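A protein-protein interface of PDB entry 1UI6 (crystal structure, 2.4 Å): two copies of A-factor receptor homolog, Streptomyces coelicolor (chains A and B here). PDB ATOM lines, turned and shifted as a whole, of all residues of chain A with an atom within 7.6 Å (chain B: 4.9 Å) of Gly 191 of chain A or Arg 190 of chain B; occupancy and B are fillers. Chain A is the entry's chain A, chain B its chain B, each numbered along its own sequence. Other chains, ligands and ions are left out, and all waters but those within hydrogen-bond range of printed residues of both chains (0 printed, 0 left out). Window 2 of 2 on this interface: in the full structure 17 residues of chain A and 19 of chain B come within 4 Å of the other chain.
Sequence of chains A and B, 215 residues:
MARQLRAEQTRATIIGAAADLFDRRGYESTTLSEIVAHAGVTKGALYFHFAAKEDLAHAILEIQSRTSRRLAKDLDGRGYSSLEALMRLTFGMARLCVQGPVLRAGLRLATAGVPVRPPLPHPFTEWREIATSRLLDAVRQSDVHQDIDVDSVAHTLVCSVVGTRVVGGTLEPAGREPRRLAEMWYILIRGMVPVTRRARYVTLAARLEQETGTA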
ATOM      1  N   VAL A 144      -7.347   8.937   1.826  1.00  0.00           N
ATOM      2  CA  VAL A 144      -6.720   7.829   2.552  1.00  0.00           C
ATOM      3  C   VAL A 144      -6.363   8.316   3.970  1.00  0.00           C
ATOM      4  O   VAL A 144      -5.804   9.384   4.130  1.00  0.00           O
ATOM      5  CB  VAL A 144      -5.403   7.433   1.888  1.00  0.00           C
ATOM      6  CG1 VAL A 144      -4.648   6.471   2.730  1.00  0.00           C
ATOM      7  CG2 VAL A 144      -5.641   6.846   0.602  1.00  0.00           C
ATOM      8  N   HIS A 145      -6.665   7.535   4.996  1.00  0.00           N
ATOM      9  CA  HIS A 145      -6.350   7.912   6.376  1.00  0.00           C
ATOM     10  C   HIS A 145      -4.936   8.429   6.556  1.00  0.00           C
ATOM     11  O   HIS A 145      -3.960   7.890   5.993  1.00  0.00           O
ATOM     12  CB  HIS A 145      -6.532   6.716   7.292  1.00  0.00           C
ATOM     13  CG  HIS A 145      -7.885   6.095   7.186  1.00  0.00           C
ATOM     14  ND1 HIS A 145      -8.077   4.738   7.052  1.00  0.00           N
ATOM     15  CD2 HIS A 145      -9.116   6.658   7.176  1.00  0.00           C
ATOM     16  CE1 HIS A 145      -9.372   4.489   6.983  1.00  0.00           C
ATOM     17  NE2 HIS A 145     -10.025   5.637   7.078  1.00  0.00           N
ATOM     18  N   ASP A 147      -3.149   8.187   9.087  1.00  0.00           N
ATOM     19  CA  ASP A 147      -2.285   7.286   9.839  1.00  0.00           C
ATOM     20  C   ASP A 147      -1.779   6.111   8.986  1.00  0.00           C
ATOM     21  O   ASP A 147      -1.005   5.294   9.458  1.00  0.00           O
ATOM     22  CB  ASP A 147      -3.052   6.730  11.065  1.00  0.00           C
ATOM     23  CG  ASP A 147      -3.135   7.713  12.216  1.00  0.00           C
ATOM     24  OD1 ASP A 147      -3.429   8.923  11.976  1.00  0.00           O
ATOM     25  OD2 ASP A 147      -2.969   7.375  13.428  1.00  0.00           O
ATOM     26  N   ILE A 148      -2.270   5.959   7.767  1.00  0.00           N
ATOM     27  CA  ILE A 148      -1.794   4.842   6.946  1.00  0.00           C
ATOM     28  C   ILE A 148      -0.292   4.957   6.668  1.00  0.00           C
ATOM     29  O   ILE A 148       0.228   6.013   6.364  1.00  0.00           O
ATOM     30  CB  ILE A 148      -2.502   4.771   5.564  1.00  0.00           C
ATOM     31  CG1 ILE A 148      -3.923   4.207   5.679  1.00  0.00           C
ATOM     32  CG2 ILE A 148      -1.681   3.979   4.596  1.00  0.00           C
ATOM     33  CD1 ILE A 148      -4.077   2.905   6.394  1.00  0.00           C
ATOM     34  N   ASP A 149       0.374   3.829   6.748  1.00  0.00           N
ATOM     35  CA  ASP A 149       1.756   3.759   6.397  1.00  0.00           C
ATOM     36  C   ASP A 149       1.827   3.481   4.877  1.00  0.00           C
ATOM     37  O   ASP A 149       1.741   2.335   4.437  1.00  0.00           O
ATOM     38  CB  ASP A 149       2.409   2.641   7.183  1.00  0.00           C
ATOM     39  CG  ASP A 149       3.890   2.592   6.976  1.00  0.00           C
ATOM     40  OD1 ASP A 149       4.497   3.668   6.954  1.00  0.00           O
ATOM     41  OD2 ASP A 149       4.546   1.551   6.831  1.00  0.00           O
ATOM     42  N   TRP A 185      -8.963  -4.063  -4.689  1.00  0.00           N
ATOM     43  CA  TRP A 185      -9.297  -2.651  -4.454  1.00  0.00           C
ATOM     44  C   TRP A 185     -10.375  -2.525  -3.422  1.00  0.00           C
ATOM     45  O   TRP A 185     -10.303  -1.655  -2.597  1.00  0.00           O
ATOM     46  CB  TRP A 185      -9.668  -1.873  -5.749  1.00  0.00           C
ATOM     47  CG  TRP A 185      -8.468  -1.316  -6.396  1.00  0.00           C
ATOM     48  CD1 TRP A 185      -7.916  -1.728  -7.545  1.00  0.00           C
ATOM     49  CD2 TRP A 185      -7.586  -0.336  -5.861  1.00  0.00           C
ATOM     50  NE1 TRP A 185      -6.747  -1.054  -7.794  1.00  0.00           N
ATOM     51  CE2 TRP A 185      -6.524  -0.187  -6.767  1.00  0.00           C
ATOM     52  CE3 TRP A 185      -7.594   0.443  -4.706  1.00  0.00           C
ATOM     53  CZ2 TRP A 185      -5.510   0.727  -6.594  1.00  0.00           C
ATOM     54  CZ3 TRP A 185      -6.564   1.340  -4.500  1.00  0.00           C
ATOM     55  CH2 TRP A 185      -5.519   1.472  -5.452  1.00  0.00           C
ATOM     56  N   TYR A 186     -11.369  -3.398  -3.432  1.00  0.00           N
ATOM     57  CA  TYR A 186     -12.440  -3.296  -2.429  1.00  0.00           C
ATOM     58  C   TYR A 186     -11.844  -3.386  -1.006  1.00  0.00           C
ATOM     59  O   TYR A 186     -12.201  -2.613  -0.117  1.00  0.00           O
ATOM     60  CB  TYR A 186     -13.523  -4.387  -2.649  1.00  0.00           C
ATOM     61  CG  TYR A 186     -14.341  -4.244  -3.952  1.00  0.00           C
ATOM     62  CD1 TYR A 186     -14.526  -3.008  -4.535  1.00  0.00           C
ATOM     63  CD2 TYR A 186     -14.885  -5.345  -4.602  1.00  0.00           C
ATOM     64  CE1 TYR A 186     -15.215  -2.845  -5.677  1.00  0.00           C
ATOM     65  CE2 TYR A 186     -15.610  -5.184  -5.804  1.00  0.00           C
ATOM     66  CZ  TYR A 186     -15.752  -3.918  -6.325  1.00  0.00           C
ATOM     67  OH  TYR A 186     -16.460  -3.653  -7.485  1.00  0.00           O
ATOM     68  N   ILE A 187     -10.927  -4.324  -0.802  1.00  0.00           N
ATOM     69  CA  ILE A 187     -10.356  -4.530   0.510  1.00  0.00           C
ATOM     70  C   ILE A 187      -9.545  -3.277   0.891  1.00  0.00           C
ATOM     71  O   ILE A 187      -9.705  -2.729   1.955  1.00  0.00           O
ATOM     72  CB  ILE A 187      -9.501  -5.826   0.505  1.00  0.00           C
ATOM     73  CG1 ILE A 187     -10.392  -7.050   0.555  1.00  0.00           C
ATOM     74  CG2 ILE A 187      -8.542  -5.851   1.647  1.00  0.00           C
ATOM     75  CD1 ILE A 187      -9.724  -8.255  -0.022  1.00  0.00           C
ATOM     76  N   LEU A 188      -8.713  -2.791  -0.002  1.00  0.00           N
ATOM     77  CA  LEU A 188      -7.964  -1.606   0.335  1.00  0.00           C
ATOM     78  C   LEU A 188      -8.923  -0.438   0.598  1.00  0.00           C
ATOM     79  O   LEU A 188      -8.676   0.411   1.479  1.00  0.00           O
ATOM     80  CB  LEU A 188      -6.975  -1.259  -0.760  1.00  0.00           C
ATOM     81  CG  LEU A 188      -5.932  -2.329  -1.118  1.00  0.00           C
ATOM     82  CD1 LEU A 188      -5.069  -1.908  -2.274  1.00  0.00           C
ATOM     83  CD2 LEU A 188      -5.017  -2.705   0.077  1.00  0.00           C
ATOM     84  N   ILE A 189     -10.023  -0.392  -0.145  1.00  0.00           N
ATOM     85  CA  ILE A 189     -10.894   0.743  -0.033  1.00  0.00           C
ATOM     86  C   ILE A 189     -11.538   0.743   1.338  1.00  0.00           C
ATOM     87  O   ILE A 189     -11.568   1.777   2.009  1.00  0.00           O
ATOM     88  CB  ILE A 189     -11.926   0.752  -1.130  1.00  0.00           C
ATOM     89  CG1 ILE A 189     -11.281   1.258  -2.414  1.00  0.00           C
ATOM     90  CG2 ILE A 189     -13.109   1.640  -0.726  1.00  0.00           C
ATOM     91  CD1 ILE A 189     -12.061   0.992  -3.603  1.00  0.00           C
ATOM     92  N   ARG A 190     -12.058  -0.410   1.739  1.00  0.00           N
ATOM     93  CA  ARG A 190     -12.656  -0.525   3.059  1.00  0.00           C
ATOM     94  C   ARG A 190     -11.619  -0.190   4.171  1.00  0.00           C
ATOM     95  O   ARG A 190     -11.923   0.481   5.137  1.00  0.00           O
ATOM     96  CB  ARG A 190     -13.211  -1.941   3.263  1.00  0.00           C
ATOM     97  CG  ARG A 190     -14.359  -2.315   2.306  1.00  0.00           C
ATOM     98  CD  ARG A 190     -15.127  -3.590   2.653  1.00  0.00           C
ATOM     99  NE  ARG A 190     -15.752  -3.536   3.973  1.00  0.00           N
ATOM    100  CZ  ARG A 190     -16.313  -4.582   4.584  1.00  0.00           C
ATOM    101  NH1 ARG A 190     -16.328  -5.773   3.990  1.00  0.00           N
ATOM    102  NH2 ARG A 190     -16.849  -4.445   5.799  1.00  0.00           N
ATOM    103  N   GLY A 191     -10.377  -0.588   3.976  1.00  0.00           N
ATOM    104  CA  GLY A 191      -9.442  -0.461   5.054  1.00  0.00           C
ATOM    105  C   GLY A 191      -8.630   0.796   5.116  1.00  0.00           C
ATOM    106  O   GLY A 191      -7.973   1.031   6.095  1.00  0.00           O
ATOM    107  N   MET A 192      -8.671   1.601   4.078  1.00  0.00           N
ATOM    108  CA  MET A 192      -7.843   2.778   4.095  1.00  0.00           C
ATOM    109  C   MET A 192      -8.584   4.050   3.700  1.00  0.00           C
ATOM    110  O   MET A 192      -8.081   5.135   3.940  1.00  0.00           O
ATOM    111  CB  MET A 192      -6.541   2.536   3.296  1.00  0.00           C
ATOM    112  CG  MET A 192      -6.593   2.633   1.805  1.00  0.00           C
ATOM    113  SD  MET A 192      -4.931   2.283   1.001  1.00  0.00           S
ATOM    114  CE  MET A 192      -4.719   0.637   1.307  1.00  0.00           C
ATOM    115  N   VAL A 193      -9.802   3.918   3.174  1.00  0.00           N
ATOM    116  CA  VAL A 193     -10.544   5.076   2.703  1.00  0.00           C
ATOM    117  C   VAL A 193     -11.612   5.469   3.701  1.00  0.00           C
ATOM    118  O   VAL A 193     -12.387   4.634   4.145  1.00  0.00           O
ATOM    119  CB  VAL A 193     -11.205   4.835   1.331  1.00  0.00           C
ATOM    120  CG1 VAL A 193     -11.910   6.035   0.867  1.00  0.00           C
ATOM    121  CG2 VAL A 193     -10.171   4.477   0.299  1.00  0.00           C
ATOM    122  N   PRO A 194     -11.641   6.750   4.060  1.00  0.00           N
ATOM    123  CA  PRO A 194     -12.688   7.235   4.974  1.00  0.00           C
ATOM    124  C   PRO A 194     -14.073   6.890   4.418  1.00  0.00           C
ATOM    125  O   PRO A 194     -14.310   6.920   3.159  1.00  0.00           O
ATOM    126  CB  PRO A 194     -12.437   8.752   5.058  1.00  0.00           C
ATOM    127  CG  PRO A 194     -10.963   8.877   4.783  1.00  0.00           C
ATOM    128  CD  PRO A 194     -10.671   7.800   3.709  1.00  0.00           C
ATOM    129  N   ARG A 198     -15.773   6.333   0.304  1.00  0.00           N
ATOM    130  CA  ARG A 198     -15.631   4.951  -0.147  1.00  0.00           C
ATOM    131  C   ARG A 198     -16.425   4.672  -1.376  1.00  0.00           C
ATOM    132  O   ARG A 198     -15.904   4.108  -2.333  1.00  0.00           O
ATOM    133  CB  ARG A 198     -16.108   3.942   0.933  1.00  0.00           C
ATOM    134  CG  ARG A 198     -15.131   3.780   2.034  1.00  0.00           C
ATOM    135  CD  ARG A 198     -15.580   2.887   3.197  1.00  0.00           C
ATOM    136  NE  ARG A 198     -14.701   3.061   4.359  1.00  0.00           N
ATOM    137  CZ  ARG A 198     -14.954   2.642   5.587  1.00  0.00           C
ATOM    138  NH1 ARG A 198     -16.075   2.014   5.867  1.00  0.00           N
ATOM    139  NH2 ARG A 198     -14.068   2.853   6.552  1.00  0.00           N
ATOM    140  N   TYR B 186      -3.741  -4.271   9.692  1.00  0.00           N
ATOM    141  CA  TYR B 186      -4.683  -3.314  10.197  1.00  0.00           C
ATOM    142  C   TYR B 186      -5.710  -3.018   9.095  1.00  0.00           C
ATOM    143  O   TYR B 186      -6.933  -2.972   9.309  1.00  0.00           O
ATOM    144  CB  TYR B 186      -3.965  -2.029  10.608  1.00  0.00           C
ATOM    145  CG  TYR B 186      -3.020  -2.121  11.770  1.00  0.00           C
ATOM    146  CD1 TYR B 186      -3.326  -2.865  12.899  1.00  0.00           C
ATOM    147  CD2 TYR B 186      -1.804  -1.424  11.767  1.00  0.00           C
ATOM    148  CE1 TYR B 186      -2.450  -2.938  13.997  1.00  0.00           C
ATOM    149  CE2 TYR B 186      -0.935  -1.508  12.832  1.00  0.00           C
ATOM    150  CZ  TYR B 186      -1.286  -2.270  13.962  1.00  0.00           C
ATOM    151  OH  TYR B 186      -0.449  -2.357  15.064  1.00  0.00           O
ATOM    152  N   ILE B 187      -5.198  -2.833   7.893  1.00  0.00           N
ATOM    153  CA  ILE B 187      -6.040  -2.503   6.751  1.00  0.00           C
ATOM    154  C   ILE B 187      -7.053  -3.633   6.515  1.00  0.00           C
ATOM    155  O   ILE B 187      -8.229  -3.378   6.379  1.00  0.00           O
ATOM    156  CB  ILE B 187      -5.170  -2.251   5.572  1.00  0.00           C
ATOM    157  CG1 ILE B 187      -4.452  -0.904   5.734  1.00  0.00           C
ATOM    158  CG2 ILE B 187      -5.971  -2.263   4.319  1.00  0.00           C
ATOM    159  CD1 ILE B 187      -3.391  -0.607   4.644  1.00  0.00           C
ATOM    160  N   LEU B 188      -6.596  -4.874   6.566  1.00  0.00           N
ATOM    161  CA  LEU B 188      -7.488  -6.019   6.372  1.00  0.00           C
ATOM    162  C   LEU B 188      -8.515  -6.127   7.490  1.00  0.00           C
ATOM    163  O   LEU B 188      -9.677  -6.384   7.219  1.00  0.00           O
ATOM    164  CB  LEU B 188      -6.714  -7.349   6.270  1.00  0.00           C
ATOM    165  CG  LEU B 188      -5.864  -7.529   5.025  1.00  0.00           C
ATOM    166  CD1 LEU B 188      -5.045  -8.801   5.125  1.00  0.00           C
ATOM    167  CD2 LEU B 188      -6.743  -7.594   3.830  1.00  0.00           C
ATOM    168  N   ILE B 189      -8.057  -5.944   8.723  1.00  0.00           N
ATOM    169  CA  ILE B 189      -8.896  -5.970   9.905  1.00  0.00           C
ATOM    170  C   ILE B 189     -10.041  -4.968   9.789  1.00  0.00           C
ATOM    171  O   ILE B 189     -11.193  -5.338  10.006  1.00  0.00           O
ATOM    172  CB  ILE B 189      -8.049  -5.696  11.190  1.00  0.00           C
ATOM    173  CG1 ILE B 189      -7.189  -6.905  11.506  1.00  0.00           C
ATOM    174  CG2 ILE B 189      -8.943  -5.413  12.401  1.00  0.00           C
ATOM    175  CD1 ILE B 189      -6.152  -6.658  12.519  1.00  0.00           C
ATOM    176  N   ARG B 190      -9.736  -3.716   9.442  1.00  0.00           N
ATOM    177  CA  ARG B 190     -10.797  -2.707   9.234  1.00  0.00           C
ATOM    178  C   ARG B 190     -11.791  -3.172   8.148  1.00  0.00           C
ATOM    179  O   ARG B 190     -12.985  -3.050   8.308  1.00  0.00           O
ATOM    180  CB  ARG B 190     -10.226  -1.321   8.888  1.00  0.00           C
ATOM    181  CG  ARG B 190      -9.725  -0.569  10.110  1.00  0.00           C
ATOM    182  CD  ARG B 190      -9.259   0.884   9.900  1.00  0.00           C
ATOM    183  NE  ARG B 190      -8.245   1.016   8.857  1.00  0.00           N
ATOM    184  CZ  ARG B 190      -6.948   1.142   9.068  1.00  0.00           C
ATOM    185  NH1 ARG B 190      -6.449   1.155  10.303  1.00  0.00           N
ATOM    186  NH2 ARG B 190      -6.142   1.246   8.025  1.00  0.00           N
ATOM    187  N   GLY B 191     -11.281  -3.782   7.094  1.00  0.00           N
ATOM    188  CA  GLY B 191     -12.113  -4.211   5.986  1.00  0.00           C
ATOM    189  C   GLY B 191     -12.763  -5.591   5.967  1.00  0.00           C
ATOM    190  O   GLY B 191     -13.617  -5.805   5.100  1.00  0.00           O
ATOM    191  N   MET B 192     -12.418  -6.501   6.886  1.00  0.00           N
ATOM    192  CA  MET B 192     -12.982  -7.860   6.857  1.00  0.00           C
ATOM    193  C   MET B 192     -13.439  -8.421   8.188  1.00  0.00           C
ATOM    194  O   MET B 192     -14.156  -9.409   8.221  1.00  0.00           O
ATOM    195  CB  MET B 192     -11.990  -8.839   6.214  1.00  0.00           C
ATOM    196  CG  MET B 192     -10.818  -9.322   7.097  1.00  0.00           C
ATOM    197  SD  MET B 192      -9.629 -10.289   6.138  1.00  0.00           S
ATOM    198  CE  MET B 192      -8.298 -10.567   7.546  1.00  0.00           C
ATOM    199  N   VAL B 193     -13.050  -7.795   9.292  1.00  0.00           N
ATOM    200  CA  VAL B 193     -13.406  -8.306  10.615  1.00  0.00           C
ATOM    201  C   VAL B 193     -14.532  -7.491  11.207  1.00  0.00           C
ATOM    202  O   VAL B 193     -14.540  -6.265  11.110  1.00  0.00           O
ATOM    203  CB  VAL B 193     -12.158  -8.265  11.552  1.00  0.00           C
ATOM    204  CG1 VAL B 193     -12.508  -8.600  12.985  1.00  0.00           C
ATOM    205  CG2 VAL B 193     -11.066  -9.186  10.989  1.00  0.00           C
ATOM    206  N   ARG B 198     -12.804  -6.619  16.256  1.00  0.00           N
ATOM    207  CA  ARG B 198     -11.597  -5.961  15.761  1.00  0.00           C
ATOM    208  C   ARG B 198     -10.503  -5.720  16.791  1.00  0.00           C
ATOM    209  O   ARG B 198      -9.372  -6.085  16.541  1.00  0.00           O
ATOM    210  CB  ARG B 198     -11.921  -4.643  15.078  1.00  0.00           C
ATOM    211  CG  ARG B 198     -12.407  -4.882  13.653  1.00  0.00           C
ATOM    212  CD  ARG B 198     -12.476  -3.642  12.790  1.00  0.00           C
ATOM    213  NE  ARG B 198     -13.591  -3.754  11.882  1.00  0.00           N
ATOM    214  CZ  ARG B 198     -14.229  -2.727  11.334  1.00  0.00           C
ATOM    215  NH1 ARG B 198     -13.857  -1.470  11.579  1.00  0.00           N
ATOM    216  NH2 ARG B 198     -15.252  -2.968  10.524  1.00  0.00           N
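The guanidinium group of Arg 190 of chain A sits at hydrogen-bond distance from the backbone carbonyl oxygen of Gly 191 of chain B. O of Gly 191 of chain A is in hydrogen-bond range of NH2 of Arg 190 of chain B (2.7 Å).
NH2 of Arg 198 of chain B sits at hydrogen-bond distance from O of Arg 190 of chain B (3.2 Å). The backbone NH (N) of His 145 of chain A lies within hydrogen-bond range of the backbone carbonyl oxygen (O) of Met 192 of chain A, at 3.0 Å. The guanidinium group (NH2) of Arg 198 of chain A sits at hydrogen-bond distance from the backbone carbonyl oxygen (O) of Arg 190 of chain A.
Among the printed residues, pairs that only touch across the chains: Ile 148 of chain A with Ile 187 of chain B, Ile 148 of chain A with Arg 190 of chain B, Ile 187 of chain A with Leu 188 of chain B, Gly 191 of chain A with Ile 187 of chain B and Met 192 of chain A with Ile 187 of chain B.
Of the printed residues of chain B, Ile 148 of chain A touches Ile 187 (3.9 Å) and Arg 190 (3.1 Å). Of chain B, only Ile 187 (3.4 Å) and Arg 190 (2.7 Å) come within 4 Å of Gly 191 of chain A. Of the printed residues of chain B, Met 192 of chain A touches Ile 187 (3.8 Å). Of the printed residues of chain A, Leu 188 of chain B touches Ile 187 (3.3 Å). Of chain A, only Ile 148 (3.1 Å) and Gly 191 (2.7 Å) come within 4 Å of Arg 190 of chain B. Of the printed residues of chain A, Gly 191 of chain B touches Arg 190. The nearest printed residue of chain B that does not touch Arg 190 of chain A is Arg 190 of chain B (4.5 Å).
Of the 9 printed residues of chain B, 4 touch a printed residue of chain A. Of the 16 printed residues of chain A, 5 touch a printed residue of chain B. Hydrophobic or aromatic side chains of chain A that line the printed part of chain B: Ile 148, Ile 187 and Met 192. Among the printed residues, no Asp or Glu carboxylate lies within 4 Å of a Lys or Arg side-chain nitrogen of the other chain.
Ile 187 of chain A touches Leu 188 of chain B, but with the chains exchanged Leu 188 of chain A does not touch Ile 187 of chain B (4.4 Å). Arg 190 of chain A touches Gly 191 of chain B, and with the chains exchanged Gly 191 of chain A touches Arg 190 of chain B. Gly 191 of chain A touches Ile 187 of chain B, but with the chains exchanged Ile 187 of chain A does not touch Gly 191 of chain B (4.9 Å). Met 192 of chain A touches Ile 187 of chain B, but with the chains exchanged Ile 187 of chain A does not touch Met 192 of chain B (6.1 Å).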
